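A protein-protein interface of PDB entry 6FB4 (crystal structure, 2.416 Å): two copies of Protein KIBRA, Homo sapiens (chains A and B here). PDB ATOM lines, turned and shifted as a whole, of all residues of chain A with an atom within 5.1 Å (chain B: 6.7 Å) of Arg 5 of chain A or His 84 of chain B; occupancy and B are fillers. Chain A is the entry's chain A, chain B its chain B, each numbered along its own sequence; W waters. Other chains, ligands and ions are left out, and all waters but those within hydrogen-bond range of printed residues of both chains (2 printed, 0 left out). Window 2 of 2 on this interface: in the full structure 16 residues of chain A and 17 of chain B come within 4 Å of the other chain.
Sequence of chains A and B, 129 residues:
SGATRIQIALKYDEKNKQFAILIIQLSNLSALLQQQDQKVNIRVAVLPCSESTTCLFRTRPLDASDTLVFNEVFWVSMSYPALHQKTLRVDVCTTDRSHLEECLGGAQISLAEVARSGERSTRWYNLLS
The side-chain amide nitrogen of Asn 126 of chain A sits at hydrogen-bond distance from the backbone carbonyl oxygen of Lys 86 of chain B, at 3.0 Å.
ND2 of Asn 126 of chain A lies close to N of Ala 112 of chain B, 3.4 Å away.
The backbone NH (N) of Ala 3 of chain A is in hydrogen-bond range of the side-chain amide oxygen (OE1) of Gln 85 of chain B (3.1 Å).
The backbone NH of Trp 124 of chain A is in hydrogen-bond range of the side-chain carboxylate of Glu 113 of chain B (2.8 Å).
OE1 of Gln 85 of chain B is in hydrogen-bond range of NH2 of Arg 5 of chain A (3.0 Å).
A ring nitrogen (ND1) of His 84 of chain B lies within hydrogen-bond range of the guanidinium group of Arg 5 of chain A.
The side-chain hydroxyl of Ser 110 of chain B lies within hydrogen-bond range of the backbone NH of Asn 126 of chain A (2.8 Å).
The side-chain amide nitrogen of Asn 126 of chain A lies within hydrogen-bond range of the backbone carbonyl oxygen of His 84 of chain B, 2.8 Å away.
N of Ser 27 of chain A lies within hydrogen-bond range of O of Arg 5 of chain A (2.9 Å).
The backbone carbonyl oxygen (O) of Pro 81 of chain B lies within hydrogen-bond range of the side-chain amide nitrogen (NE2) of Gln 85 of chain B (3.0 Å).
OH of Tyr 80 of chain B sits close to NE2 of His 84 of chain B, 3.2 Å away.
O of Lys 86 of chain B is in hydrogen-bond range of N of Leu 111 of chain B (3.1 Å).
The backbone carbonyl oxygen (O) of Ile 6 of chain A is in hydrogen-bond range of the backbone NH (N) of Tyr 125 of chain A.
The guanidinium group of Arg 5 of chain A sits at hydrogen-bond distance from the side-chain amide oxygen of Asn 126 of chain A.
Among the printed residues, merely in contact across the chains: Asn 126 of chain A with Gln 85 of chain B, Tyr 125 of chain A with Ser 110 of chain B and Trp 124 of chain A with Ala 112 of chain B.
Printed residues of chain B within 4 Å of Arg 5 of chain A: His 84 (3.0 Å) and Gln 85 (3.0 Å).
Of the printed residues of chain B, Asn 126 of chain A touches His 84, Gln 85, Lys 86, Ser 110 and Ala 112.
Pro 81 of chain B touches none of the printed residues of chain A.
Printed residues of chain A within 4 Å of Lys 86 of chain B: Asn 126.
Of the printed residues of chain A, Ser 110 of chain B touches Tyr 125 and Asn 126.
Leu 111 of chain B touches none of the printed residues of chain A.
Of the printed residues of chain A, Ala 112 of chain B touches Trp 124 (3.8 Å) and Asn 126 (3.4 Å).
Printed residues of chain A within 4 Å of Glu 113 of chain B: Trp 124.
The nearest printed residue of chain B that does not touch Arg 5 of chain A is Ala 112 of chain B (4.01 Å).
Of the 14 printed residues of chain B, 6 touch a printed residue of chain A.
Printed residues of chain B that touch a printed residue of chain A: His 84, Gln 85, Lys 86, Ser 110, Ala 112 and Glu 113.
Hydrophobic or aromatic side chains of chain B within 4 Å of the printed part of chain A: His 84 and Ala 112.
Of the 12 printed residues of chain A, 5 touch a printed residue of chain B.
Printed residues of chain A that touch a printed residue of chain B: Ala 3, Arg 5, Trp 124, Tyr 125 and Asn 126.
Hydrophobic or aromatic side chains of chain A that line the printed part of chain B: Ala 3 and Trp 124.
Along chain A the printed residues that touch a printed residue of chain B span positions 3 to 126.
Among the printed residues, 11 pairs touch across the chains.
Among the printed residues, no Asp or Glu carboxylate lies within 4 Å of a Lys or Arg side-chain nitrogen of the other chain.
No position is printed for both chains.
Of the 11 pairs that touch across the chains among the printed residues, none has its exchanged pair printed and touching as well.
Water W2 lies within hydrogen-bond range of the side-chain hydroxyl of Ser 110 of chain B and the backbone carbonyl oxygen of Trp 124 of chain A.
Water W1 lies within hydrogen-bond range of O of Gln 85 of chain B (2.9 Å) and O of Leu 127 of chain A (3.5 Å).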
ATOM      1  N   ALA A   3      -8.692  -5.040 -14.419  1.00  0.00           N
ATOM      2  CA  ALA A   3     -10.022  -5.332 -14.929  1.00  0.00           C
ATOM      3  C   ALA A   3     -10.041  -5.196 -16.447  1.00  0.00           C
ATOM      4  O   ALA A   3      -9.415  -4.298 -17.012  1.00  0.00           O
ATOM      5  CB  ALA A   3     -11.074  -4.405 -14.304  1.00  0.00           C
ATOM      6  N   THR A   4     -10.749  -6.113 -17.095  1.00  0.00           N
ATOM      7  CA  THR A   4     -11.113  -5.949 -18.489  1.00  0.00           C
ATOM      8  C   THR A   4     -12.281  -4.994 -18.571  1.00  0.00           C
ATOM      9  O   THR A   4     -13.184  -5.020 -17.730  1.00  0.00           O
ATOM     10  CB  THR A   4     -11.492  -7.284 -19.120  1.00  0.00           C
ATOM     11  OG1 THR A   4     -10.427  -8.213 -18.935  1.00  0.00           O
ATOM     12  CG2 THR A   4     -11.730  -7.122 -20.606  1.00  0.00           C
ATOM     13  N   ARG A   5     -12.257  -4.140 -19.585  1.00  0.00           N
ATOM     14  CA  ARG A   5     -13.263  -3.112 -19.735  1.00  0.00           C
ATOM     15  C   ARG A   5     -13.835  -3.155 -21.135  1.00  0.00           C
ATOM     16  O   ARG A   5     -13.172  -3.556 -22.100  1.00  0.00           O
ATOM     17  CB  ARG A   5     -12.703  -1.719 -19.470  1.00  0.00           C
ATOM     18  CG  ARG A   5     -12.155  -1.529 -18.078  1.00  0.00           C
ATOM     19  CD  ARG A   5     -11.834  -0.074 -17.822  1.00  0.00           C
ATOM     20  NE  ARG A   5     -11.484   0.129 -16.422  1.00  0.00           N
ATOM     21  CZ  ARG A   5     -10.251   0.025 -15.930  1.00  0.00           C
ATOM     22  NH1 ARG A   5      -9.219  -0.277 -16.716  1.00  0.00           N
ATOM     23  NH2 ARG A   5     -10.047   0.221 -14.639  1.00  0.00           N
ATOM     24  N   ILE A   6     -15.080  -2.731 -21.225  1.00  0.00           N
ATOM     25  CA  ILE A   6     -15.764  -2.614 -22.492  1.00  0.00           C
ATOM     26  C   ILE A   6     -16.299  -1.197 -22.592  1.00  0.00           C
ATOM     27  O   ILE A   6     -16.803  -0.634 -21.613  1.00  0.00           O
ATOM     28  CB  ILE A   6     -16.875  -3.674 -22.622  1.00  0.00           C
ATOM     29  CG1 ILE A   6     -17.451  -3.656 -24.036  1.00  0.00           C
ATOM     30  CG2 ILE A   6     -17.932  -3.467 -21.559  1.00  0.00           C
ATOM     31  CD1 ILE A   6     -18.483  -4.712 -24.288  1.00  0.00           C
ATOM     32  N   GLN A   7     -16.144  -0.599 -23.761  1.00  0.00           N
ATOM     33  CA  GLN A   7     -16.645   0.738 -24.006  1.00  0.00           C
ATOM     34  C   GLN A   7     -17.900   0.620 -24.851  1.00  0.00           C
ATOM     35  O   GLN A   7     -17.888  -0.045 -25.895  1.00  0.00           O
ATOM     36  CB  GLN A   7     -15.593   1.601 -24.703  1.00  0.00           C
ATOM     37  CG  GLN A   7     -15.999   3.046 -24.793  1.00  0.00           C
ATOM     38  CD  GLN A   7     -15.046   3.853 -25.613  1.00  0.00           C
ATOM     39  OE1 GLN A   7     -14.628   3.436 -26.700  1.00  0.00           O
ATOM     40  NE2 GLN A   7     -14.680   5.022 -25.098  1.00  0.00           N
ATOM     41  N   GLN A  25     -15.461  -1.408 -28.064  1.00  0.00           N
ATOM     42  CA  GLN A  25     -14.174  -2.071 -27.904  1.00  0.00           C
ATOM     43  C   GLN A  25     -13.978  -2.655 -26.511  1.00  0.00           C
ATOM     44  O   GLN A  25     -14.663  -2.302 -25.550  1.00  0.00           O
ATOM     45  CB  GLN A  25     -13.035  -1.100 -28.186  1.00  0.00           C
ATOM     46  CG  GLN A  25     -13.025   0.103 -27.267  1.00  0.00           C
ATOM     47  CD  GLN A  25     -11.818   0.974 -27.480  1.00  0.00           C
ATOM     48  OE1 GLN A  25     -10.747   0.482 -27.852  1.00  0.00           O
ATOM     49  NE2 GLN A  25     -11.977   2.278 -27.261  1.00  0.00           N
ATOM     50  N   LEU A  26     -12.989  -3.539 -26.431  1.00  0.00           N
ATOM     51  CA  LEU A  26     -12.491  -4.115 -25.197  1.00  0.00           C
ATOM     52  C   LEU A  26     -11.088  -3.619 -24.926  1.00  0.00           C
ATOM     53  O   LEU A  26     -10.285  -3.472 -25.850  1.00  0.00           O
ATOM     54  CB  LEU A  26     -12.434  -5.635 -25.289  1.00  0.00           C
ATOM     55  CG  LEU A  26     -13.786  -6.280 -25.519  1.00  0.00           C
ATOM     56  CD1 LEU A  26     -13.573  -7.735 -25.864  1.00  0.00           C
ATOM     57  CD2 LEU A  26     -14.677  -6.111 -24.281  1.00  0.00           C
ATOM     58  N   SER A  27     -10.774  -3.408 -23.663  1.00  0.00           N
ATOM     59  CA  SER A  27      -9.410  -3.100 -23.285  1.00  0.00           C
ATOM     60  C   SER A  27      -8.964  -4.067 -22.202  1.00  0.00           C
ATOM     61  O   SER A  27      -9.778  -4.609 -21.447  1.00  0.00           O
ATOM     62  CB  SER A  27      -9.268  -1.663 -22.802  1.00  0.00           C
ATOM     63  OG  SER A  27      -9.671  -1.550 -21.449  1.00  0.00           O
ATOM     64  N   TRP A 124     -17.112   3.567 -20.173  1.00  0.00           N
ATOM     65  CA  TRP A 124     -16.386   2.331 -19.964  1.00  0.00           C
ATOM     66  C   TRP A 124     -16.994   1.565 -18.793  1.00  0.00           C
ATOM     67  O   TRP A 124     -17.382   2.160 -17.787  1.00  0.00           O
ATOM     68  CB  TRP A 124     -14.920   2.612 -19.666  1.00  0.00           C
ATOM     69  CG  TRP A 124     -14.047   3.023 -20.826  1.00  0.00           C
ATOM     70  CD1 TRP A 124     -13.682   4.295 -21.173  1.00  0.00           C
ATOM     71  CD2 TRP A 124     -13.397   2.154 -21.760  1.00  0.00           C
ATOM     72  NE1 TRP A 124     -12.859   4.272 -22.275  1.00  0.00           N
ATOM     73  CE2 TRP A 124     -12.663   2.969 -22.649  1.00  0.00           C
ATOM     74  CE3 TRP A 124     -13.366   0.770 -21.933  1.00  0.00           C
ATOM     75  CZ2 TRP A 124     -11.916   2.441 -23.689  1.00  0.00           C
ATOM     76  CZ3 TRP A 124     -12.627   0.250 -22.965  1.00  0.00           C
ATOM     77  CH2 TRP A 124     -11.907   1.079 -23.827  1.00  0.00           C
ATOM     78  N   TYR A 125     -17.055   0.236 -18.917  1.00  0.00           N
ATOM     79  CA  TYR A 125     -17.672  -0.603 -17.904  1.00  0.00           C
ATOM     80  C   TYR A 125     -16.732  -1.747 -17.548  1.00  0.00           C
ATOM     81  O   TYR A 125     -16.206  -2.427 -18.432  1.00  0.00           O
ATOM     82  CB  TYR A 125     -19.018  -1.146 -18.384  1.00  0.00           C
ATOM     83  CG  TYR A 125     -20.010  -0.070 -18.767  1.00  0.00           C
ATOM     84  CD1 TYR A 125     -20.051   0.451 -20.058  1.00  0.00           C
ATOM     85  CD2 TYR A 125     -20.904   0.428 -17.835  1.00  0.00           C
ATOM     86  CE1 TYR A 125     -20.954   1.445 -20.402  1.00  0.00           C
ATOM     87  CE2 TYR A 125     -21.806   1.417 -18.165  1.00  0.00           C
ATOM     88  CZ  TYR A 125     -21.828   1.921 -19.446  1.00  0.00           C
ATOM     89  OH  TYR A 125     -22.742   2.896 -19.756  1.00  0.00           O
ATOM     90  N   ASN A 126     -16.514  -1.946 -16.251  1.00  0.00           N
ATOM     91  CA  ASN A 126     -15.723  -3.066 -15.795  1.00  0.00           C
ATOM     92  C   ASN A 126     -16.485  -4.357 -16.021  1.00  0.00           C
ATOM     93  O   ASN A 126     -17.710  -4.415 -15.885  1.00  0.00           O
ATOM     94  CB  ASN A 126     -15.369  -2.909 -14.323  1.00  0.00           C
ATOM     95  CG  ASN A 126     -14.307  -1.855 -14.102  1.00  0.00           C
ATOM     96  OD1 ASN A 126     -13.469  -1.633 -14.973  1.00  0.00           O
ATOM     97  ND2 ASN A 126     -14.340  -1.186 -12.947  1.00  0.00           N
ATOM     98  N   LEU A 127     -15.754  -5.388 -16.403  1.00  0.00           N
ATOM     99  CA  LEU A 127     -16.322  -6.716 -16.492  1.00  0.00           C
ATOM    100  C   LEU A 127     -16.095  -7.445 -15.178  1.00  0.00           C
ATOM    101  O   LEU A 127     -15.035  -7.331 -14.555  1.00  0.00           O
ATOM    102  CB  LEU A 127     -15.696  -7.490 -17.651  1.00  0.00           C
ATOM    103  CG  LEU A 127     -15.844  -6.848 -19.026  1.00  0.00           C
ATOM    104  CD1 LEU A 127     -15.348  -7.791 -20.049  1.00  0.00           C
ATOM    105  CD2 LEU A 127     -17.282  -6.502 -19.336  1.00  0.00           C
ATOM    106  N   MET B  78      -9.671   1.965   0.047  1.00  0.00           N
ATOM    107  CA  MET B  78      -8.871   1.525  -1.087  1.00  0.00           C
ATOM    108  C   MET B  78      -8.531   2.710  -1.962  1.00  0.00           C
ATOM    109  O   MET B  78      -9.291   3.675  -2.059  1.00  0.00           O
ATOM    110  CB  MET B  78      -9.580   0.458  -1.921  1.00  0.00           C
ATOM    111  CG  MET B  78     -10.892   0.867  -2.533  1.00  0.00           C
ATOM    112  SD  MET B  78     -11.758  -0.618  -3.131  1.00  0.00           S
ATOM    113  CE  MET B  78     -10.442  -1.467  -3.959  1.00  0.00           C
ATOM    114  N   SER B  79      -7.383   2.606  -2.611  1.00  0.00           N
ATOM    115  CA  SER B  79      -6.910   3.668  -3.479  1.00  0.00           C
ATOM    116  C   SER B  79      -7.796   3.776  -4.712  1.00  0.00           C
ATOM    117  O   SER B  79      -8.423   2.803  -5.138  1.00  0.00           O
ATOM    118  CB  SER B  79      -5.485   3.375  -3.910  1.00  0.00           C
ATOM    119  OG  SER B  79      -5.506   2.255  -4.777  1.00  0.00           O
ATOM    120  N   TYR B  80      -7.836   4.966  -5.298  1.00  0.00           N
ATOM    121  CA  TYR B  80      -8.619   5.136  -6.512  1.00  0.00           C
ATOM    122  C   TYR B  80      -8.269   4.110  -7.576  1.00  0.00           C
ATOM    123  O   TYR B  80      -9.193   3.573  -8.198  1.00  0.00           O
ATOM    124  CB  TYR B  80      -8.446   6.541  -7.084  1.00  0.00           C
ATOM    125  CG  TYR B  80      -9.222   6.696  -8.349  1.00  0.00           C
ATOM    126  CD1 TYR B  80     -10.597   6.891  -8.318  1.00  0.00           C
ATOM    127  CD2 TYR B  80      -8.591   6.628  -9.583  1.00  0.00           C
ATOM    128  CE1 TYR B  80     -11.322   7.023  -9.490  1.00  0.00           C
ATOM    129  CE2 TYR B  80      -9.302   6.758 -10.759  1.00  0.00           C
ATOM    130  CZ  TYR B  80     -10.667   6.956 -10.713  1.00  0.00           C
ATOM    131  OH  TYR B  80     -11.361   7.077 -11.898  1.00  0.00           O
ATOM    132  N   PRO B  81      -6.999   3.803  -7.832  1.00  0.00           N
ATOM    133  CA  PRO B  81      -6.691   2.813  -8.879  1.00  0.00           C
ATOM    134  C   PRO B  81      -7.346   1.467  -8.649  1.00  0.00           C
ATOM    135  O   PRO B  81      -7.874   0.859  -9.584  1.00  0.00           O
ATOM    136  CB  PRO B  81      -5.159   2.712  -8.818  1.00  0.00           C
ATOM    137  CG  PRO B  81      -4.705   3.985  -8.195  1.00  0.00           C
ATOM    138  CD  PRO B  81      -5.788   4.424  -7.273  1.00  0.00           C
ATOM    139  N   ALA B  82      -7.314   0.970  -7.423  1.00  0.00           N
ATOM    140  CA  ALA B  82      -7.992  -0.281  -7.129  1.00  0.00           C
ATOM    141  C   ALA B  82      -9.505  -0.145  -7.293  1.00  0.00           C
ATOM    142  O   ALA B  82     -10.149  -1.021  -7.873  1.00  0.00           O
ATOM    143  CB  ALA B  82      -7.646  -0.724  -5.710  1.00  0.00           C
ATOM    144  N   LEU B  83     -10.086   0.941  -6.774  1.00  0.00           N
ATOM    145  CA  LEU B  83     -11.522   1.162  -6.893  1.00  0.00           C
ATOM    146  C   LEU B  83     -11.957   1.173  -8.348  1.00  0.00           C
ATOM    147  O   LEU B  83     -13.054   0.721  -8.689  1.00  0.00           O
ATOM    148  CB  LEU B  83     -11.898   2.485  -6.235  1.00  0.00           C
ATOM    149  CG  LEU B  83     -13.374   2.848  -6.394  1.00  0.00           C
ATOM    150  CD1 LEU B  83     -14.182   1.906  -5.543  1.00  0.00           C
ATOM    151  CD2 LEU B  83     -13.660   4.286  -6.026  1.00  0.00           C
ATOM    152  N   HIS B  84     -11.122   1.726  -9.211  1.00  0.00           N
ATOM    153  CA  HIS B  84     -11.436   1.851 -10.619  1.00  0.00           C
ATOM    154  C   HIS B  84     -11.603   0.498 -11.317  1.00  0.00           C
ATOM    155  O   HIS B  84     -12.149   0.455 -12.423  1.00  0.00           O
ATOM    156  CB  HIS B  84     -10.325   2.682 -11.247  1.00  0.00           C
ATOM    157  CG  HIS B  84     -10.736   3.389 -12.481  1.00  0.00           C
ATOM    158  ND1 HIS B  84     -10.229   3.072 -13.725  1.00  0.00           N
ATOM    159  CD2 HIS B  84     -11.617   4.394 -12.672  1.00  0.00           C
ATOM    160  CE1 HIS B  84     -10.780   3.856 -14.631  1.00  0.00           C
ATOM    161  NE2 HIS B  84     -11.624   4.670 -14.018  1.00  0.00           N
ATOM    162  N   GLN B  85     -11.165  -0.597 -10.694  1.00  0.00           N
ATOM    163  CA  GLN B  85     -11.291  -1.937 -11.243  1.00  0.00           C
ATOM    164  C   GLN B  85     -12.497  -2.687 -10.712  1.00  0.00           C
ATOM    165  O   GLN B  85     -12.738  -3.819 -11.141  1.00  0.00           O
ATOM    166  CB  GLN B  85     -10.042  -2.770 -10.929  1.00  0.00           C
ATOM    167  CG  GLN B  85      -8.723  -2.022 -10.994  1.00  0.00           C
ATOM    168  CD  GLN B  85      -8.433  -1.454 -12.363  1.00  0.00           C
ATOM    169  OE1 GLN B  85      -8.708  -2.098 -13.378  1.00  0.00           O
ATOM    170  NE2 GLN B  85      -7.869  -0.237 -12.404  1.00  0.00           N
ATOM    171  N   LYS B  86     -13.253  -2.106  -9.793  1.00  0.00           N
ATOM    172  CA  LYS B  86     -14.218  -2.884  -9.042  1.00  0.00           C
ATOM    173  C   LYS B  86     -15.605  -2.731  -9.633  1.00  0.00           C
ATOM    174  O   LYS B  86     -15.860  -1.902 -10.508  1.00  0.00           O
ATOM    175  CB  LYS B  86     -14.229  -2.472  -7.569  1.00  0.00           C
ATOM    176  CG  LYS B  86     -12.895  -2.624  -6.852  1.00  0.00           C
ATOM    177  CD  LYS B  86     -12.421  -4.067  -6.845  1.00  0.00           C
ATOM    178  CE  LYS B  86     -11.293  -4.300  -5.842  1.00  0.00           C
ATOM    179  NZ  LYS B  86     -10.858  -5.722  -5.737  1.00  0.00           N
ATOM    180  N   SER B 110     -20.743  -1.001 -12.374  1.00  0.00           N
ATOM    181  CA  SER B 110     -19.344  -0.765 -12.652  1.00  0.00           C
ATOM    182  C   SER B 110     -18.883   0.526 -12.000  1.00  0.00           C
ATOM    183  O   SER B 110     -19.515   1.575 -12.153  1.00  0.00           O
ATOM    184  CB  SER B 110     -19.149  -0.694 -14.166  1.00  0.00           C
ATOM    185  OG  SER B 110     -17.834  -0.303 -14.465  1.00  0.00           O
ATOM    186  N   LEU B 111     -17.768   0.452 -11.285  1.00  0.00           N
ATOM    187  CA  LEU B 111     -17.171   1.628 -10.661  1.00  0.00           C
ATOM    188  C   LEU B 111     -16.074   2.255 -11.512  1.00  0.00           C
ATOM    189  O   LEU B 111     -15.381   3.159 -11.044  1.00  0.00           O
ATOM    190  CB  LEU B 111     -16.629   1.252  -9.284  1.00  0.00           C
ATOM    191  CG  LEU B 111     -17.714   0.694  -8.344  1.00  0.00           C
ATOM    192  CD1 LEU B 111     -17.114   0.334  -7.024  1.00  0.00           C
ATOM    193  CD2 LEU B 111     -18.848   1.682  -8.132  1.00  0.00           C
ATOM    194  N   ALA B 112     -15.914   1.807 -12.758  1.00  0.00           N
ATOM    195  CA  ALA B 112     -14.870   2.338 -13.625  1.00  0.00           C
ATOM    196  C   ALA B 112     -14.989   3.842 -13.837  1.00  0.00           C
ATOM    197  O   ALA B 112     -14.009   4.483 -14.201  1.00  0.00           O
ATOM    198  CB  ALA B 112     -14.910   1.629 -14.979  1.00  0.00           C
ATOM    199  N   GLU B 113     -16.154   4.426 -13.615  1.00  0.00           N
ATOM    200  CA  GLU B 113     -16.383   5.808 -14.000  1.00  0.00           C
ATOM    201  C   GLU B 113     -16.671   6.709 -12.791  1.00  0.00           C
ATOM    202  O   GLU B 113     -17.196   7.816 -12.953  1.00  0.00           O
ATOM    203  CB  GLU B 113     -17.510   5.843 -15.034  1.00  0.00           C
ATOM    204  CG  GLU B 113     -17.223   6.756 -16.205  1.00  0.00           C
ATOM    205  CD  GLU B 113     -16.413   6.100 -17.283  1.00  0.00           C
ATOM    206  OE1 GLU B 113     -17.016   5.644 -18.267  1.00  0.00           O
ATOM    207  OE2 GLU B 113     -15.171   6.040 -17.163  1.00  0.00           O
ATOM    208  N   VAL B 114     -16.339   6.240 -11.580  1.00  0.00           N
ATOM    209  CA  VAL B 114     -16.341   7.071 -10.375  1.00  0.00           C
ATOM    210  C   VAL B 114     -15.215   8.094 -10.461  1.00  0.00           C
ATOM    211  O   VAL B 114     -14.066   7.747 -10.755  1.00  0.00           O
ATOM    212  CB  VAL B 114     -16.172   6.205  -9.117  1.00  0.00           C
ATOM    213  CG1 VAL B 114     -15.984   7.058  -7.908  1.00  0.00           C
ATOM    214  CG2 VAL B 114     -17.355   5.311  -8.889  1.00  0.00           C
HETATM  215  O   HOH W   1     -15.217  -5.292 -11.733  1.00  0.00           O
HETATM  216  O   HOH W   2     -18.575   2.258 -15.245  1.00  0.00           O
